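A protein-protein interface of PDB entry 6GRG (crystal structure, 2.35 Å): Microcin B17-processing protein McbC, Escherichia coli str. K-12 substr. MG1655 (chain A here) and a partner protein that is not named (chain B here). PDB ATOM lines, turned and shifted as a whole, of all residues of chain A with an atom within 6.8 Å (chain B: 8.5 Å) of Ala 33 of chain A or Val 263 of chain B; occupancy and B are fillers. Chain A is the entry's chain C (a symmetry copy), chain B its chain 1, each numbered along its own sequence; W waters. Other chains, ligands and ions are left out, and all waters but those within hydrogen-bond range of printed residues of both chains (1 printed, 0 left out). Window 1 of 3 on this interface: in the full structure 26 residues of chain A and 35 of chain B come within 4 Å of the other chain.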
ATOM      1  N   ASN A  31     -22.923  25.013  27.547  1.00  0.00           N
ATOM      2  CA  ASN A  31     -22.558  24.053  28.601  1.00  0.00           C
ATOM      3  C   ASN A  31     -21.146  23.508  28.357  1.00  0.00           C
ATOM      4  O   ASN A  31     -20.729  23.304  27.182  1.00  0.00           O
ATOM      5  CB  ASN A  31     -23.499  22.860  28.704  1.00  0.00           C
ATOM      6  CG  ASN A  31     -24.871  23.212  29.248  1.00  0.00           C
ATOM      7  OD1 ASN A  31     -25.061  24.220  29.926  1.00  0.00           O
ATOM      8  ND2 ASN A  31     -25.837  22.361  28.955  1.00  0.00           N
ATOM      9  N   PHE A  32     -20.475  23.180  29.468  1.00  0.00           N
ATOM     10  CA  PHE A  32     -19.105  22.687  29.475  1.00  0.00           C
ATOM     11  C   PHE A  32     -19.056  21.227  29.924  1.00  0.00           C
ATOM     12  O   PHE A  32     -19.863  20.811  30.718  1.00  0.00           O
ATOM     13  CB  PHE A  32     -18.235  23.497  30.445  1.00  0.00           C
ATOM     14  CG  PHE A  32     -17.579  24.735  29.891  1.00  0.00           C
ATOM     15  CD1 PHE A  32     -17.969  25.292  28.680  1.00  0.00           C
ATOM     16  CD2 PHE A  32     -16.567  25.359  30.605  1.00  0.00           C
ATOM     17  CE1 PHE A  32     -17.365  26.442  28.198  1.00  0.00           C
ATOM     18  CE2 PHE A  32     -15.973  26.518  30.127  1.00  0.00           C
ATOM     19  CZ  PHE A  32     -16.368  27.049  28.922  1.00  0.00           C
ATOM     20  N   ALA A  33     -18.064  20.502  29.396  1.00  0.00           N
ATOM     21  CA  ALA A  33     -17.636  19.192  29.838  1.00  0.00           C
ATOM     22  C   ALA A  33     -16.239  19.359  30.444  1.00  0.00           C
ATOM     23  O   ALA A  33     -15.212  19.185  29.777  1.00  0.00           O
ATOM     24  CB  ALA A  33     -17.628  18.216  28.684  1.00  0.00           C
ATOM     25  N   SER A  34     -16.239  19.755  31.715  1.00  0.00           N
ATOM     26  CA  SER A  34     -15.083  20.147  32.449  1.00  0.00           C
ATOM     27  C   SER A  34     -14.901  19.176  33.624  1.00  0.00           C
ATOM     28  O   SER A  34     -15.655  19.213  34.588  1.00  0.00           O
ATOM     29  CB  SER A  34     -15.272  21.573  32.884  1.00  0.00           C
ATOM     30  OG  SER A  34     -14.192  22.003  33.687  1.00  0.00           O
ATOM     31  N   LEU A  35     -13.881  18.322  33.518  1.00  0.00           N
ATOM     32  CA  LEU A  35     -13.613  17.192  34.397  1.00  0.00           C
ATOM     33  C   LEU A  35     -12.108  16.974  34.502  1.00  0.00           C
ATOM     34  O   LEU A  35     -11.415  17.035  33.500  1.00  0.00           O
ATOM     35  CB  LEU A  35     -14.230  15.929  33.784  1.00  0.00           C
ATOM     36  CG  LEU A  35     -15.739  15.738  33.907  1.00  0.00           C
ATOM     37  CD1 LEU A  35     -16.112  14.318  33.504  1.00  0.00           C
ATOM     38  CD2 LEU A  35     -16.226  16.032  35.326  1.00  0.00           C
ATOM     39  N   PHE A  38     -10.658  14.777  31.700  1.00  0.00           N
ATOM     40  CA  PHE A  38     -10.646  15.302  30.312  1.00  0.00           C
ATOM     41  C   PHE A  38      -9.583  16.399  30.095  1.00  0.00           C
ATOM     42  O   PHE A  38      -9.472  16.934  28.990  1.00  0.00           O
ATOM     43  CB  PHE A  38     -12.019  15.854  29.920  1.00  0.00           C
ATOM     44  CG  PHE A  38     -13.166  14.878  29.961  1.00  0.00           C
ATOM     45  CD1 PHE A  38     -12.958  13.505  29.904  1.00  0.00           C
ATOM     46  CD2 PHE A  38     -14.470  15.342  30.047  1.00  0.00           C
ATOM     47  CE1 PHE A  38     -14.031  12.626  29.945  1.00  0.00           C
ATOM     48  CE2 PHE A  38     -15.541  14.463  30.100  1.00  0.00           C
ATOM     49  CZ  PHE A  38     -15.318  13.106  30.033  1.00  0.00           C
ATOM     50  N   THR A  42      -8.933  18.252  26.267  1.00  0.00           N
ATOM     51  CA  THR A  42      -9.846  19.337  26.031  1.00  0.00           C
ATOM     52  C   THR A  42      -9.143  20.662  26.293  1.00  0.00           C
ATOM     53  O   THR A  42      -8.049  20.696  26.847  1.00  0.00           O
ATOM     54  CB  THR A  42     -11.113  19.235  26.887  1.00  0.00           C
ATOM     55  OG1 THR A  42     -10.759  19.145  28.264  1.00  0.00           O
ATOM     56  CG2 THR A  42     -11.975  18.053  26.504  1.00  0.00           C
ATOM     57  N   PHE A  43      -9.788  21.756  25.902  1.00  0.00           N
ATOM     58  CA  PHE A  43      -9.308  23.049  26.373  1.00  0.00           C
ATOM     59  C   PHE A  43     -10.488  23.998  26.623  1.00  0.00           C
ATOM     60  O   PHE A  43     -11.616  23.706  26.228  1.00  0.00           O
ATOM     61  CB  PHE A  43      -8.294  23.613  25.382  1.00  0.00           C
ATOM     62  CG  PHE A  43      -8.912  24.088  24.103  1.00  0.00           C
ATOM     63  CD1 PHE A  43      -9.170  23.196  23.075  1.00  0.00           C
ATOM     64  CD2 PHE A  43      -9.274  25.415  23.942  1.00  0.00           C
ATOM     65  CE1 PHE A  43      -9.726  23.632  21.886  1.00  0.00           C
ATOM     66  CE2 PHE A  43      -9.847  25.845  22.756  1.00  0.00           C
ATOM     67  CZ  PHE A  43     -10.064  24.953  21.730  1.00  0.00           C
ATOM     68  N   VAL A  44     -10.202  25.119  27.291  1.00  0.00           N
ATOM     69  CA  VAL A  44     -11.210  26.132  27.617  1.00  0.00           C
ATOM     70  C   VAL A  44     -11.020  27.423  26.796  1.00  0.00           C
ATOM     71  O   VAL A  44     -12.035  27.965  26.301  1.00  0.00           O
ATOM     72  CB  VAL A  44     -11.271  26.433  29.125  1.00  0.00           C
ATOM     73  CG1 VAL A  44     -12.371  27.443  29.411  1.00  0.00           C
ATOM     74  CG2 VAL A  44     -11.528  25.178  29.927  1.00  0.00           C
ATOM     75  N   SER A  45      -9.768  27.921  26.700  1.00  0.00           N
ATOM     76  CA  SER A  45      -9.445  29.254  26.173  1.00  0.00           C
ATOM     77  C   SER A  45      -9.088  29.138  24.692  1.00  0.00           C
ATOM     78  O   SER A  45      -8.233  28.335  24.354  1.00  0.00           O
ATOM     79  CB  SER A  45      -8.311  29.873  26.971  1.00  0.00           C
ATOM     80  OG  SER A  45      -7.896  31.129  26.445  1.00  0.00           O
ATOM     81  N   TYR A 238     -17.356  24.364  35.383  1.00  0.00           N
ATOM     82  CA  TYR A 238     -18.056  23.203  35.868  1.00  0.00           C
ATOM     83  C   TYR A 238     -18.825  22.554  34.709  1.00  0.00           C
ATOM     84  O   TYR A 238     -19.154  23.209  33.733  1.00  0.00           O
ATOM     85  CB  TYR A 238     -18.924  23.598  37.071  1.00  0.00           C
ATOM     86  CG  TYR A 238     -20.056  24.524  36.721  1.00  0.00           C
ATOM     87  CD1 TYR A 238     -21.245  24.016  36.251  1.00  0.00           C
ATOM     88  CD2 TYR A 238     -19.918  25.896  36.804  1.00  0.00           C
ATOM     89  CE1 TYR A 238     -22.297  24.847  35.910  1.00  0.00           C
ATOM     90  CE2 TYR A 238     -20.952  26.744  36.457  1.00  0.00           C
ATOM     91  CZ  TYR A 238     -22.147  26.216  35.997  1.00  0.00           C
ATOM     92  OH  TYR A 238     -23.203  27.007  35.649  1.00  0.00           O
ATOM     93  N   THR A 239     -19.088  21.253  34.852  1.00  0.00           N
ATOM     94  CA  THR A 239     -19.932  20.521  33.935  1.00  0.00           C
ATOM     95  C   THR A 239     -21.404  20.688  34.329  1.00  0.00           C
ATOM     96  O   THR A 239     -21.878  20.082  35.304  1.00  0.00           O
ATOM     97  CB  THR A 239     -19.580  19.032  33.906  1.00  0.00           C
ATOM     98  OG1 THR A 239     -18.180  18.913  33.695  1.00  0.00           O
ATOM     99  CG2 THR A 239     -20.337  18.310  32.818  1.00  0.00           C
ATOM    100  N   ASP A 240     -22.131  21.453  33.516  1.00  0.00           N
ATOM    101  CA  ASP A 240     -23.468  21.931  33.840  1.00  0.00           C
ATOM    102  C   ASP A 240     -24.406  20.779  34.250  1.00  0.00           C
ATOM    103  O   ASP A 240     -25.115  20.843  35.295  1.00  0.00           O
ATOM    104  CB  ASP A 240     -24.009  22.717  32.665  1.00  0.00           C
ATOM    105  CG  ASP A 240     -23.186  23.962  32.413  1.00  0.00           C
ATOM    106  OD1 ASP A 240     -21.985  23.814  32.023  1.00  0.00           O
ATOM    107  OD2 ASP A 240     -23.737  25.070  32.643  1.00  0.00           O
ATOM    108  N   LEU B 188     -23.109  11.742  34.552  1.00  0.00           N
ATOM    109  CA  LEU B 188     -22.869  13.158  34.186  1.00  0.00           C
ATOM    110  C   LEU B 188     -24.171  13.902  33.838  1.00  0.00           C
ATOM    111  O   LEU B 188     -24.170  15.130  33.780  1.00  0.00           O
ATOM    112  CB  LEU B 188     -21.855  13.221  33.032  1.00  0.00           C
ATOM    113  CG  LEU B 188     -20.430  12.795  33.406  1.00  0.00           C
ATOM    114  CD1 LEU B 188     -19.522  12.738  32.190  1.00  0.00           C
ATOM    115  CD2 LEU B 188     -19.843  13.725  34.461  1.00  0.00           C
ATOM    116  N   THR B 190     -26.225  13.387  30.967  1.00  0.00           N
ATOM    117  CA  THR B 190     -26.261  13.812  29.578  1.00  0.00           C
ATOM    118  C   THR B 190     -27.386  13.120  28.815  1.00  0.00           C
ATOM    119  O   THR B 190     -27.778  12.005  29.107  1.00  0.00           O
ATOM    120  CB  THR B 190     -24.924  13.593  28.851  1.00  0.00           C
ATOM    121  OG1 THR B 190     -24.637  12.202  28.842  1.00  0.00           O
ATOM    122  CG2 THR B 190     -23.764  14.336  29.471  1.00  0.00           C
ATOM    123  N   LEU B 253     -12.218  10.707  22.687  1.00  0.00           N
ATOM    124  CA  LEU B 253     -12.747  10.488  24.043  1.00  0.00           C
ATOM    125  C   LEU B 253     -11.739   9.716  24.890  1.00  0.00           C
ATOM    126  O   LEU B 253     -11.518  10.108  26.030  1.00  0.00           O
ATOM    127  CB  LEU B 253     -14.072   9.719  23.983  1.00  0.00           C
ATOM    128  CG  LEU B 253     -15.258  10.455  23.356  1.00  0.00           C
ATOM    129  CD1 LEU B 253     -16.292   9.455  22.880  1.00  0.00           C
ATOM    130  CD2 LEU B 253     -15.887  11.417  24.342  1.00  0.00           C
ATOM    131  N   LYS B 260      -6.948  18.758  20.581  1.00  0.00           N
ATOM    132  CA  LYS B 260      -7.833  18.966  21.721  1.00  0.00           C
ATOM    133  C   LYS B 260      -9.183  19.540  21.276  1.00  0.00           C
ATOM    134  O   LYS B 260      -9.243  20.410  20.397  1.00  0.00           O
ATOM    135  CB  LYS B 260      -7.181  19.924  22.718  1.00  0.00           C
ATOM    136  CG  LYS B 260      -5.939  19.379  23.411  1.00  0.00           C
ATOM    137  CD  LYS B 260      -5.706  20.017  24.757  1.00  0.00           C
ATOM    138  CE  LYS B 260      -4.521  19.433  25.492  1.00  0.00           C
ATOM    139  NZ  LYS B 260      -3.247  19.832  24.853  1.00  0.00           N
ATOM    140  N   SER B 261     -10.257  19.039  21.902  1.00  0.00           N
ATOM    141  CA  SER B 261     -11.629  19.536  21.703  1.00  0.00           C
ATOM    142  C   SER B 261     -11.939  20.627  22.731  1.00  0.00           C
ATOM    143  O   SER B 261     -11.474  20.531  23.839  1.00  0.00           O
ATOM    144  CB  SER B 261     -12.621  18.434  21.808  1.00  0.00           C
ATOM    145  OG  SER B 261     -12.546  17.614  20.665  1.00  0.00           O
ATOM    146  N   HIS B 262     -12.707  21.658  22.339  1.00  0.00           N
ATOM    147  CA  HIS B 262     -13.240  22.616  23.314  1.00  0.00           C
ATOM    148  C   HIS B 262     -14.257  21.908  24.223  1.00  0.00           C
ATOM    149  O   HIS B 262     -15.028  21.021  23.789  1.00  0.00           O
ATOM    150  CB  HIS B 262     -13.858  23.865  22.667  1.00  0.00           C
ATOM    151  CG  HIS B 262     -14.004  25.003  23.626  1.00  0.00           C
ATOM    152  ND1 HIS B 262     -15.185  25.276  24.277  1.00  0.00           N
ATOM    153  CD2 HIS B 262     -13.106  25.898  24.091  1.00  0.00           C
ATOM    154  CE1 HIS B 262     -15.019  26.311  25.078  1.00  0.00           C
ATOM    155  NE2 HIS B 262     -13.751  26.703  24.996  1.00  0.00           N
ATOM    156  N   VAL B 263     -14.264  22.350  25.483  1.00  0.00           N
ATOM    157  CA  VAL B 263     -15.088  21.797  26.541  1.00  0.00           C
ATOM    158  C   VAL B 263     -16.578  21.913  26.168  1.00  0.00           C
ATOM    159  O   VAL B 263     -17.380  21.059  26.594  1.00  0.00           O
ATOM    160  CB  VAL B 263     -14.772  22.439  27.910  1.00  0.00           C
ATOM    161  CG1 VAL B 263     -13.444  21.942  28.462  1.00  0.00           C
ATOM    162  CG2 VAL B 263     -14.778  23.952  27.872  1.00  0.00           C
ATOM    163  N   ASP B 264     -16.943  22.897  25.329  1.00  0.00           N
ATOM    164  CA  ASP B 264     -18.377  23.154  25.030  1.00  0.00           C
ATOM    165  C   ASP B 264     -18.973  22.180  23.995  1.00  0.00           C
ATOM    166  O   ASP B 264     -20.191  22.249  23.747  1.00  0.00           O
ATOM    167  CB  ASP B 264     -18.663  24.613  24.645  1.00  0.00           C
ATOM    168  CG  ASP B 264     -18.120  25.131  23.320  1.00  0.00           C
ATOM    169  OD1 ASP B 264     -17.646  24.311  22.508  1.00  0.00           O
ATOM    170  OD2 ASP B 264     -18.179  26.379  23.110  1.00  0.00           O
ATOM    171  N   ASN B 265     -18.127  21.331  23.385  1.00  0.00           N
ATOM    172  CA  ASN B 265     -18.520  20.435  22.277  1.00  0.00           C
ATOM    173  C   ASN B 265     -18.035  18.992  22.493  1.00  0.00           C
ATOM    174  O   ASN B 265     -18.489  18.075  21.811  1.00  0.00           O
ATOM    175  CB  ASN B 265     -18.042  20.962  20.918  1.00  0.00           C
ATOM    176  CG  ASN B 265     -16.535  21.024  20.750  1.00  0.00           C
ATOM    177  OD1 ASN B 265     -15.832  20.020  20.876  1.00  0.00           O
ATOM    178  ND2 ASN B 265     -16.037  22.206  20.424  1.00  0.00           N
ATOM    179  N   PHE B 266     -17.188  18.767  23.498  1.00  0.00           N
ATOM    180  CA  PHE B 266     -16.421  17.508  23.646  1.00  0.00           C
ATOM    181  C   PHE B 266     -17.337  16.267  23.631  1.00  0.00           C
ATOM    182  O   PHE B 266     -16.986  15.247  23.045  1.00  0.00           O
ATOM    183  CB  PHE B 266     -15.542  17.589  24.895  1.00  0.00           C
ATOM    184  CG  PHE B 266     -14.748  16.345  25.180  1.00  0.00           C
ATOM    185  CD1 PHE B 266     -13.789  15.892  24.282  1.00  0.00           C
ATOM    186  CD2 PHE B 266     -14.955  15.624  26.349  1.00  0.00           C
ATOM    187  CE1 PHE B 266     -13.065  14.737  24.545  1.00  0.00           C
ATOM    188  CE2 PHE B 266     -14.221  14.474  26.616  1.00  0.00           C
ATOM    189  CZ  PHE B 266     -13.296  14.024  25.706  1.00  0.00           C
ATOM    190  N   MET B 267     -18.535  16.376  24.203  1.00  0.00           N
ATOM    191  CA  MET B 267     -19.418  15.230  24.368  1.00  0.00           C
ATOM    192  C   MET B 267     -20.616  15.227  23.398  1.00  0.00           C
ATOM    193  O   MET B 267     -21.400  14.286  23.399  1.00  0.00           O
ATOM    194  CB  MET B 267     -19.867  15.199  25.825  1.00  0.00           C
ATOM    195  CG  MET B 267     -18.773  14.568  26.654  1.00  0.00           C
ATOM    196  SD  MET B 267     -19.215  14.379  28.340  1.00  0.00           S
ATOM    197  CE  MET B 267     -20.319  12.971  28.269  1.00  0.00           C
ATOM    198  N   SER B 268     -20.680  16.223  22.510  1.00  0.00           N
ATOM    199  CA  SER B 268     -21.805  16.468  21.634  1.00  0.00           C
ATOM    200  C   SER B 268     -21.916  15.417  20.535  1.00  0.00           C
ATOM    201  O   SER B 268     -20.968  14.680  20.226  1.00  0.00           O
ATOM    202  CB  SER B 268     -21.680  17.818  20.989  1.00  0.00           C
ATOM    203  OG  SER B 268     -21.579  18.832  21.961  1.00  0.00           O
ATOM    204  N   PRO B 283     -24.649  20.066  20.223  1.00  0.00           N
ATOM    205  CA  PRO B 283     -25.185  19.576  21.482  1.00  0.00           C
ATOM    206  C   PRO B 283     -26.722  19.618  21.429  1.00  0.00           C
ATOM    207  O   PRO B 283     -27.312  20.616  21.049  1.00  0.00           O
ATOM    208  CB  PRO B 283     -24.548  20.527  22.499  1.00  0.00           C
ATOM    209  CG  PRO B 283     -24.540  21.833  21.767  1.00  0.00           C
ATOM    210  CD  PRO B 283     -24.287  21.480  20.316  1.00  0.00           C
HETATM  211  O   HOH W   1     -22.467  22.172  24.945  1.00  0.00           O
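Printed residues of chain B that touch a printed residue of chain A: Leu 188, Lys 260, Ser 261, His 262, Val 263, Asp 264 and Phe 266. Hydrophobic or aromatic side chains of chain B within 4 Å of the printed part of chain A: Leu 188, His 262, Val 263 and Phe 266. Along chain B the printed residues that touch a printed residue of chain A span positions 188 to 266. Hydrophobic or aromatic side chains of chain A within 4 Å of the printed part of chain B: Phe 32, Ala 33, Leu 35, Phe 38 and Phe 43. Along chain A the printed residues that touch a printed residue of chain B span positions 31 to 44. Among the printed residues, 15 pairs touch across the chains. Among the printed residues, no Asp or Glu carboxylate lies within 4 Å of a Lys or Arg side-chain nitrogen of the other chain.
The backbone carbonyl oxygen (O) of Ser 261 of chain B lies within hydrogen-bond range of the backbone NH (N) of Phe 43 of chain A, 2.9 Å away. A ring nitrogen (NE2) of His 262 of chain B sits at hydrogen-bond distance from the backbone carbonyl oxygen (O) of Val 44 of chain A (2.5 Å). The backbone carbonyl oxygen (O) of Val 263 of chain B sits at hydrogen-bond distance from the backbone NH (N) of Ala 33 of chain A (2.9 Å). N of Val 263 of chain B sits at hydrogen-bond distance from O of Phe 43 of chain A (3.1 Å).
Among the printed residues, merely in contact across the chains: Asn 31 of chain A with Asp 264 of chain B, Phe 32 of chain A with His 262 of chain B, Phe 32 of chain A with Val 263 of chain B, Leu 35 of chain A with Leu 188 of chain B, Phe 38 of chain A with Phe 266 of chain B, Thr 42 of chain A with Lys 260 of chain B, Thr 42 of chain A with Ser 261 of chain B, Thr 42 of chain A with Val 263 of chain B, Thr 42 of chain A with Phe 266 of chain B, Phe 43 of chain A with Lys 260 of chain B and Phe 43 of chain A with His 262 of chain B.
Water W1 bridges the backbone carbonyl oxygen (O) of Asp 264 of chain B (2.6 Å) and the backbone carbonyl oxygen (O) of Asn 31 of chain A (3.1 Å).
Printed residues of chain B within 4 Å of Asn 31 of chain A: Asp 264 (3.2 Å). Of chain B, only His 262 (3.9 Å) and Val 263 (3.5 Å) come within 4 Å of Phe 32 of chain A. Of chain B, only Val 263 (2.9 Å) comes within 4 Å of Ala 33 of chain A. Of the printed residues of chain B, Phe 43 of chain A touches Lys 260 (3.6 Å), Ser 261 (2.9 Å), His 262 (3.4 Å) and Val 263 (3.1 Å). Ser 45 of chain A touches none of the printed residues of chain B. Val 263 of chain B touches four residues of chain A. The nearest residue of chain B that does not touch Ala 33 of chain A is Met 267 of chain B (4.2 Å). The nearest printed residue of chain B that does not touch Asn 31 of chain A is Val 263 of chain B (4.1 Å).
ND1 of His 262 of chain B lies close to N of Asp 264 of chain B (3.1 Å). O of His 262 of chain B lies close to OD1 of Asn 265 of chain B, at 3.2 Å. ND2 of Asn 265 of chain B is in hydrogen-bond range of OD1 of Asp 264 of chain B. OD1 of Asn 31 of chain A sits close to OD2 of Asp 240 of chain A (3.1 Å). The backbone NH (N) of Phe 32 of chain A is in hydrogen-bond range of the side-chain carboxylate (OD1) of Asp 240 of chain A (3.0 Å). The backbone carbonyl oxygen (O) of Phe 38 of chain A is in hydrogen-bond range of the side-chain hydroxyl (OG1) of Thr 42 of chain A (2.7 Å).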
